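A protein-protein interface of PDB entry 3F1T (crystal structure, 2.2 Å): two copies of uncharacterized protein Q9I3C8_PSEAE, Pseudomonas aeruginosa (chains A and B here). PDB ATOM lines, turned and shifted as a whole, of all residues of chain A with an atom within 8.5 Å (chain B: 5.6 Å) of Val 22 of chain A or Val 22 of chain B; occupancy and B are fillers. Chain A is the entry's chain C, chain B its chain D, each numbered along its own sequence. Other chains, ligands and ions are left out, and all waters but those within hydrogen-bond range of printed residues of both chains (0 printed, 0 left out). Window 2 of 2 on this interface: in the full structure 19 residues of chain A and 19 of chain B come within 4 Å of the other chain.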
ATOM      1  N   LEU A  17     -18.790 -13.114  17.661  1.00  0.00           N
ATOM      2  CA  LEU A  17     -19.965 -13.896  18.040  1.00  0.00           C
ATOM      3  C   LEU A  17     -19.948 -14.192  19.534  1.00  0.00           C
ATOM      4  O   LEU A  17     -19.500 -15.258  19.957  1.00  0.00           O
ATOM      5  CB  LEU A  17     -20.050 -15.186  17.218  1.00  0.00           C
ATOM      6  CG  LEU A  17     -20.632 -15.036  15.804  1.00  0.00           C
ATOM      7  CD1 LEU A  17     -20.277 -13.701  15.187  1.00  0.00           C
ATOM      8  CD2 LEU A  17     -20.234 -16.176  14.877  1.00  0.00           C
ATOM      9  N   ARG A  18     -20.357 -13.203  20.328  1.00  0.00           N
ATOM     10  CA  ARG A  18     -20.067 -13.176  21.766  1.00  0.00           C
ATOM     11  C   ARG A  18     -20.726 -14.340  22.498  1.00  0.00           C
ATOM     12  O   ARG A  18     -20.425 -14.605  23.664  1.00  0.00           O
ATOM     13  CB  ARG A  18     -20.535 -11.857  22.392  1.00  0.00           C
ATOM     14  CG  ARG A  18     -19.691 -10.634  22.025  1.00  0.00           C
ATOM     15  CD  ARG A  18     -18.241 -10.779  22.490  1.00  0.00           C
ATOM     16  NE  ARG A  18     -18.158 -11.098  23.916  1.00  0.00           N
ATOM     17  CZ  ARG A  18     -17.017 -11.197  24.594  1.00  0.00           C
ATOM     18  NH1 ARG A  18     -15.854 -10.975  23.979  1.00  0.00           N
ATOM     19  NH2 ARG A  18     -17.035 -11.521  25.887  1.00  0.00           N
ATOM     20  N   HIS A  19     -21.691 -14.974  21.840  1.00  0.00           N
ATOM     21  CA  HIS A  19     -22.538 -15.961  22.503  1.00  0.00           C
ATOM     22  C   HIS A  19     -22.111 -17.403  22.225  1.00  0.00           C
ATOM     23  O   HIS A  19     -22.377 -18.295  23.033  1.00  0.00           O
ATOM     24  CB  HIS A  19     -24.018 -15.747  22.157  1.00  0.00           C
ATOM     25  CG  HIS A  19     -24.347 -15.974  20.713  1.00  0.00           C
ATOM     26  ND1 HIS A  19     -24.330 -14.960  19.778  1.00  0.00           N
ATOM     27  CD2 HIS A  19     -24.769 -17.084  20.058  1.00  0.00           C
ATOM     28  CE1 HIS A  19     -24.661 -15.451  18.596  1.00  0.00           C
ATOM     29  NE2 HIS A  19     -24.913 -16.742  18.735  1.00  0.00           N
ATOM     30  N   CYS A  20     -21.417 -17.620  21.109  1.00  0.00           N
ATOM     31  CA  CYS A  20     -20.718 -18.886  20.866  1.00  0.00           C
ATOM     32  C   CYS A  20     -19.512 -19.016  21.775  1.00  0.00           C
ATOM     33  O   CYS A  20     -18.811 -20.032  21.735  1.00  0.00           O
ATOM     34  CB  CYS A  20     -20.233 -18.972  19.418  1.00  0.00           C
ATOM     35  SG  CYS A  20     -21.432 -18.460  18.195  1.00  0.00           S
ATOM     36  N   GLN A  21     -19.115 -17.899  22.373  1.00  0.00           N
ATOM     37  CA  GLN A  21     -17.854 -17.856  23.083  1.00  0.00           C
ATOM     38  C   GLN A  21     -17.796 -19.032  24.058  1.00  0.00           C
ATOM     39  O   GLN A  21     -16.773 -19.713  24.172  1.00  0.00           O
ATOM     40  CB  GLN A  21     -17.722 -16.527  23.828  1.00  0.00           C
ATOM     41  CG  GLN A  21     -16.285 -16.177  24.199  1.00  0.00           C
ATOM     42  CD  GLN A  21     -16.211 -14.948  25.090  1.00  0.00           C
ATOM     43  OE1 GLN A  21     -16.799 -14.913  26.177  1.00  0.00           O
ATOM     44  NE2 GLN A  21     -15.464 -13.937  24.642  1.00  0.00           N
ATOM     45  N   VAL A  22     -18.949 -19.351  24.638  1.00  0.00           N
ATOM     46  CA  VAL A  22     -19.077 -20.425  25.625  1.00  0.00           C
ATOM     47  C   VAL A  22     -18.634 -21.786  25.090  1.00  0.00           C
ATOM     48  O   VAL A  22     -18.363 -22.692  25.871  1.00  0.00           O
ATOM     49  CB  VAL A  22     -20.541 -20.578  26.083  1.00  0.00           C
ATOM     50  CG1 VAL A  22     -20.605 -21.380  27.384  1.00  0.00           C
ATOM     51  CG2 VAL A  22     -21.204 -19.201  26.228  1.00  0.00           C
ATOM     52  N   LEU A  23     -18.783 -21.981  23.781  1.00  0.00           N
ATOM     53  CA  LEU A  23     -18.523 -23.266  23.139  1.00  0.00           C
ATOM     54  C   LEU A  23     -17.047 -23.511  22.808  1.00  0.00           C
ATOM     55  O   LEU A  23     -16.671 -24.628  22.469  1.00  0.00           O
ATOM     56  CB  LEU A  23     -19.371 -23.416  21.874  1.00  0.00           C
ATOM     57  CG  LEU A  23     -20.892 -23.377  22.021  1.00  0.00           C
ATOM     58  CD1 LEU A  23     -21.551 -23.511  20.674  1.00  0.00           C
ATOM     59  CD2 LEU A  23     -21.364 -24.491  22.931  1.00  0.00           C
ATOM     60  N   GLY A  24     -16.213 -22.478  22.905  1.00  0.00           N
ATOM     61  CA  GLY A  24     -14.784 -22.623  22.607  1.00  0.00           C
ATOM     62  C   GLY A  24     -14.511 -22.972  21.155  1.00  0.00           C
ATOM     63  O   GLY A  24     -13.620 -23.768  20.844  1.00  0.00           O
ATOM     64  N   LEU A  25     -15.393 -22.511  20.278  1.00  0.00           N
ATOM     65  CA  LEU A  25     -15.249 -22.724  18.848  1.00  0.00           C
ATOM     66  C   LEU A  25     -13.950 -22.103  18.346  1.00  0.00           C
ATOM     67  O   LEU A  25     -13.588 -20.997  18.744  1.00  0.00           O
ATOM     68  CB  LEU A  25     -16.439 -22.097  18.117  1.00  0.00           C
ATOM     69  CG  LEU A  25     -17.617 -22.977  17.684  1.00  0.00           C
ATOM     70  CD1 LEU A  25     -18.020 -24.012  18.704  1.00  0.00           C
ATOM     71  CD2 LEU A  25     -18.811 -22.120  17.257  1.00  0.00           C
ATOM     72  N   LEU A  39     -15.678 -27.637  17.123  1.00  0.00           N
ATOM     73  CA  LEU A  39     -16.300 -27.612  18.451  1.00  0.00           C
ATOM     74  C   LEU A  39     -15.619 -28.604  19.402  1.00  0.00           C
ATOM     75  O   LEU A  39     -15.663 -29.800  19.182  1.00  0.00           O
ATOM     76  CB  LEU A  39     -17.792 -27.953  18.329  1.00  0.00           C
ATOM     77  CG  LEU A  39     -18.523 -28.301  19.623  1.00  0.00           C
ATOM     78  CD1 LEU A  39     -18.687 -27.049  20.481  1.00  0.00           C
ATOM     79  CD2 LEU A  39     -19.874 -28.943  19.326  1.00  0.00           C
ATOM     80  N   PRO A  40     -14.949 -28.111  20.448  1.00  0.00           N
ATOM     81  CA  PRO A  40     -14.370 -29.123  21.321  1.00  0.00           C
ATOM     82  C   PRO A  40     -15.442 -29.712  22.213  1.00  0.00           C
ATOM     83  O   PRO A  40     -16.264 -28.978  22.758  1.00  0.00           O
ATOM     84  CB  PRO A  40     -13.364 -28.338  22.167  1.00  0.00           C
ATOM     85  CG  PRO A  40     -13.893 -26.949  22.192  1.00  0.00           C
ATOM     86  CD  PRO A  40     -14.642 -26.740  20.888  1.00  0.00           C
ATOM     87  N   SER A  42     -15.688 -30.984  25.136  1.00  0.00           N
ATOM     88  CA  SER A  42     -15.784 -30.662  26.552  1.00  0.00           C
ATOM     89  C   SER A  42     -16.656 -29.434  26.797  1.00  0.00           C
ATOM     90  O   SER A  42     -17.039 -29.163  27.923  1.00  0.00           O
ATOM     91  CB  SER A  42     -14.393 -30.423  27.133  1.00  0.00           C
ATOM     92  OG  SER A  42     -13.766 -29.323  26.491  1.00  0.00           O
ATOM     93  N   GLN A  43     -16.936 -28.672  25.746  1.00  0.00           N
ATOM     94  CA  GLN A  43     -17.630 -27.392  25.891  1.00  0.00           C
ATOM     95  C   GLN A  43     -19.120 -27.490  25.553  1.00  0.00           C
ATOM     96  O   GLN A  43     -19.877 -26.543  25.782  1.00  0.00           O
ATOM     97  CB  GLN A  43     -16.951 -26.311  25.041  1.00  0.00           C
ATOM     98  CG  GLN A  43     -15.659 -25.760  25.659  1.00  0.00           C
ATOM     99  CD  GLN A  43     -15.832 -25.350  27.118  1.00  0.00           C
ATOM    100  OE1 GLN A  43     -16.766 -24.628  27.468  1.00  0.00           O
ATOM    101  NE2 GLN A  43     -14.908 -25.778  27.967  1.00  0.00           N
ATOM    102  N   ALA A  44     -19.553 -28.677  25.129  1.00  0.00           N
ATOM    103  CA  ALA A  44     -20.919 -28.876  24.654  1.00  0.00           C
ATOM    104  C   ALA A  44     -21.605 -30.090  25.282  1.00  0.00           C
ATOM    105  O   ALA A  44     -22.439 -30.729  24.640  1.00  0.00           O
ATOM    106  CB  ALA A  44     -20.935 -28.994  23.141  1.00  0.00           C
ATOM    107  N   ILE A  45     -21.263 -30.399  26.533  1.00  0.00           N
ATOM    108  CA  ILE A  45     -21.691 -31.654  27.163  1.00  0.00           C
ATOM    109  C   ILE A  45     -23.132 -31.580  27.651  1.00  0.00           C
ATOM    110  O   ILE A  45     -23.520 -30.620  28.323  1.00  0.00           O
ATOM    111  CB  ILE A  45     -20.810 -32.062  28.376  1.00  0.00           C
ATOM    112  CG1 ILE A  45     -19.338 -32.238  27.968  1.00  0.00           C
ATOM    113  CG2 ILE A  45     -21.348 -33.341  29.007  1.00  0.00           C
ATOM    114  CD1 ILE A  45     -19.073 -33.399  27.038  1.00  0.00           C
ATOM    115  N   ALA A  58     -25.377 -27.625  20.303  1.00  0.00           N
ATOM    116  CA  ALA A  58     -24.030 -27.090  20.075  1.00  0.00           C
ATOM    117  C   ALA A  58     -23.561 -27.315  18.637  1.00  0.00           C
ATOM    118  O   ALA A  58     -22.888 -26.471  18.032  1.00  0.00           O
ATOM    119  CB  ALA A  58     -23.051 -27.711  21.058  1.00  0.00           C
ATOM    120  N   ARG B  18     -26.606 -24.788  28.625  1.00  0.00           N
ATOM    121  CA  ARG B  18     -25.606 -23.773  28.979  1.00  0.00           C
ATOM    122  C   ARG B  18     -25.708 -22.541  28.077  1.00  0.00           C
ATOM    123  O   ARG B  18     -25.821 -21.405  28.564  1.00  0.00           O
ATOM    124  CB  ARG B  18     -24.202 -24.362  28.831  1.00  0.00           C
ATOM    125  CG  ARG B  18     -23.825 -24.648  27.366  1.00  0.00           C
ATOM    126  CD  ARG B  18     -24.185 -26.084  26.954  1.00  0.00           C
ATOM    127  NE  ARG B  18     -25.118 -26.124  25.823  1.00  0.00           N
ATOM    128  CZ  ARG B  18     -24.846 -25.656  24.604  1.00  0.00           C
ATOM    129  NH1 ARG B  18     -23.696 -25.031  24.380  1.00  0.00           N
ATOM    130  NH2 ARG B  18     -25.741 -25.763  23.626  1.00  0.00           N
ATOM    131  N   HIS B  19     -25.510 -22.771  26.776  1.00  0.00           N
ATOM    132  CA  HIS B  19     -25.580 -21.725  25.760  1.00  0.00           C
ATOM    133  C   HIS B  19     -26.830 -20.870  25.956  1.00  0.00           C
ATOM    134  O   HIS B  19     -26.784 -19.644  25.866  1.00  0.00           O
ATOM    135  CB  HIS B  19     -25.582 -22.355  24.356  1.00  0.00           C
ATOM    136  CG  HIS B  19     -25.309 -21.384  23.245  1.00  0.00           C
ATOM    137  ND1 HIS B  19     -25.498 -20.017  23.382  1.00  0.00           N
ATOM    138  CD2 HIS B  19     -24.950 -21.592  21.950  1.00  0.00           C
ATOM    139  CE1 HIS B  19     -25.216 -19.422  22.235  1.00  0.00           C
ATOM    140  NE2 HIS B  19     -24.854 -20.351  21.360  1.00  0.00           N
ATOM    141  N   CYS B  20     -27.933 -21.525  26.287  1.00  0.00           N
ATOM    142  CA  CYS B  20     -29.175 -20.823  26.532  1.00  0.00           C
ATOM    143  C   CYS B  20     -29.125 -19.868  27.721  1.00  0.00           C
ATOM    144  O   CYS B  20     -29.682 -18.772  27.671  1.00  0.00           O
ATOM    145  CB  CYS B  20     -30.294 -21.828  26.694  1.00  0.00           C
ATOM    146  SG  CYS B  20     -30.623 -22.626  25.134  1.00  0.00           S
ATOM    147  N   GLN B  21     -28.379 -20.254  28.750  1.00  0.00           N
ATOM    148  CA  GLN B  21     -28.213 -19.421  29.938  1.00  0.00           C
ATOM    149  C   GLN B  21     -27.311 -18.219  29.678  1.00  0.00           C
ATOM    150  O   GLN B  21     -27.573 -17.131  30.178  1.00  0.00           O
ATOM    151  CB  GLN B  21     -27.699 -20.252  31.119  1.00  0.00           C
ATOM    152  CG  GLN B  21     -28.700 -21.314  31.595  1.00  0.00           C
ATOM    153  CD  GLN B  21     -30.097 -20.743  31.830  1.00  0.00           C
ATOM    154  OE1 GLN B  21     -30.245 -19.614  32.308  1.00  0.00           O
ATOM    155  NE2 GLN B  21     -31.128 -21.535  31.523  1.00  0.00           N
ATOM    156  N   VAL B  22     -26.312 -18.389  28.818  1.00  0.00           N
ATOM    157  CA  VAL B  22     -25.536 -17.247  28.339  1.00  0.00           C
ATOM    158  C   VAL B  22     -26.368 -16.282  27.492  1.00  0.00           C
ATOM    159  O   VAL B  22     -26.245 -15.062  27.618  1.00  0.00           O
ATOM    160  CB  VAL B  22     -24.293 -17.693  27.549  1.00  0.00           C
ATOM    161  CG1 VAL B  22     -23.311 -16.526  27.401  1.00  0.00           C
ATOM    162  CG2 VAL B  22     -23.634 -18.866  28.253  1.00  0.00           C
ATOM    163  N   LEU B  23     -27.240 -16.831  26.656  1.00  0.00           N
ATOM    164  CA  LEU B  23     -28.190 -16.018  25.915  1.00  0.00           C
ATOM    165  C   LEU B  23     -29.188 -15.348  26.861  1.00  0.00           C
ATOM    166  O   LEU B  23     -29.837 -14.379  26.500  1.00  0.00           O
ATOM    167  CB  LEU B  23     -28.929 -16.882  24.893  1.00  0.00           C
ATOM    168  CG  LEU B  23     -28.567 -16.755  23.410  1.00  0.00           C
ATOM    169  CD1 LEU B  23     -27.403 -15.820  23.163  1.00  0.00           C
ATOM    170  CD2 LEU B  23     -28.300 -18.115  22.815  1.00  0.00           C
ATOM    171  N   GLY B  24     -29.362 -15.922  28.047  1.00  0.00           N
ATOM    172  CA  GLY B  24     -30.375 -15.453  28.984  1.00  0.00           C
ATOM    173  C   GLY B  24     -31.795 -15.756  28.548  1.00  0.00           C
ATOM    174  O   GLY B  24     -32.699 -14.973  28.795  1.00  0.00           O
ATOM    175  N   GLN B  43     -28.367  -9.670  24.989  1.00  0.00           N
ATOM    176  CA  GLN B  43     -27.547 -10.873  24.958  1.00  0.00           C
ATOM    177  C   GLN B  43     -27.356 -11.399  23.526  1.00  0.00           C
ATOM    178  O   GLN B  43     -26.598 -12.350  23.291  1.00  0.00           O
ATOM    179  CB  GLN B  43     -28.180 -11.946  25.851  1.00  0.00           C
ATOM    180  CG  GLN B  43     -28.359 -11.514  27.308  1.00  0.00           C
ATOM    181  CD  GLN B  43     -27.043 -11.107  27.960  1.00  0.00           C
ATOM    182  OE1 GLN B  43     -26.026 -11.788  27.807  1.00  0.00           O
ATOM    183  NE2 GLN B  43     -27.049  -9.972  28.662  1.00  0.00           N
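Val 22 of chain B touches one residue of chain A.
Of the printed residues of chain B, Leu 23 of chain A touches Arg 18.
Printed residues of chain B within 4 Å of Ala 58 of chain A: Arg 18 (3.8 Å).
Cys 20 of chain B touches none of the printed residues of chain A.
Leu 39 of chain A touches none of the printed residues of chain B.
The nearest residue of chain B that does not touch Val 22 of chain A is Arg 18 of chain B (4.6 Å).
The nearest residue of chain A that does not touch Val 22 of chain B is His 19 of chain A (4.8 Å).
The nearest printed residue of chain A that does not touch Arg 18 of chain B is Gln 43 of chain A (4.3 Å).
OE1 of Gln 43 of chain A lies close to O of Val 22 of chain A, 3.0 Å away.
The backbone carbonyl oxygen (O) of Val 22 of chain B lies close to the side-chain amide oxygen (OE1) of Gln 43 of chain B, 3.3 Å away.
Of the 16 printed residues of chain A, 4 touch a printed residue of chain B.
Hydrophobic or aromatic side chains of chain B that line the printed part of chain A: His 19, Val 22 and Leu 23.
Among the printed residues, no Asp or Glu carboxylate lies within 4 Å of a Lys or Arg side-chain nitrogen of the other chain.
His 19 of chain A touches its own counterpart, His 19 of chain B.
His 19 of chain A touches Leu 23 of chain B, but with the chains exchanged Leu 23 of chain A does not touch His 19 of chain B (4.1 Å).
Val 22 of chain A touches its own counterpart, Val 22 of chain B.
Leu 23 of chain A touches Arg 18 of chain B, but with the chains exchanged Arg 18 of chain A does not touch Leu 23 of chain B (6.9 Å).
8 positions are printed for both chains.
Of the 5 pairs that touch across the chains among the printed residues, 2 have their exchanged pair printed and touching as well.
His 19 of chain B touches His 19 of chain A (CE1 to O, 3.2 Å).
Leu 23 of chain B touches His 19 of chain A.
Val 22 of chain A touches Val 22 of chain B.
Leu 23 of chain A touches Arg 18 of chain B.
NH2 of Arg 18 of chain B touches N of Ala 58 of chain A (3.8 Å).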
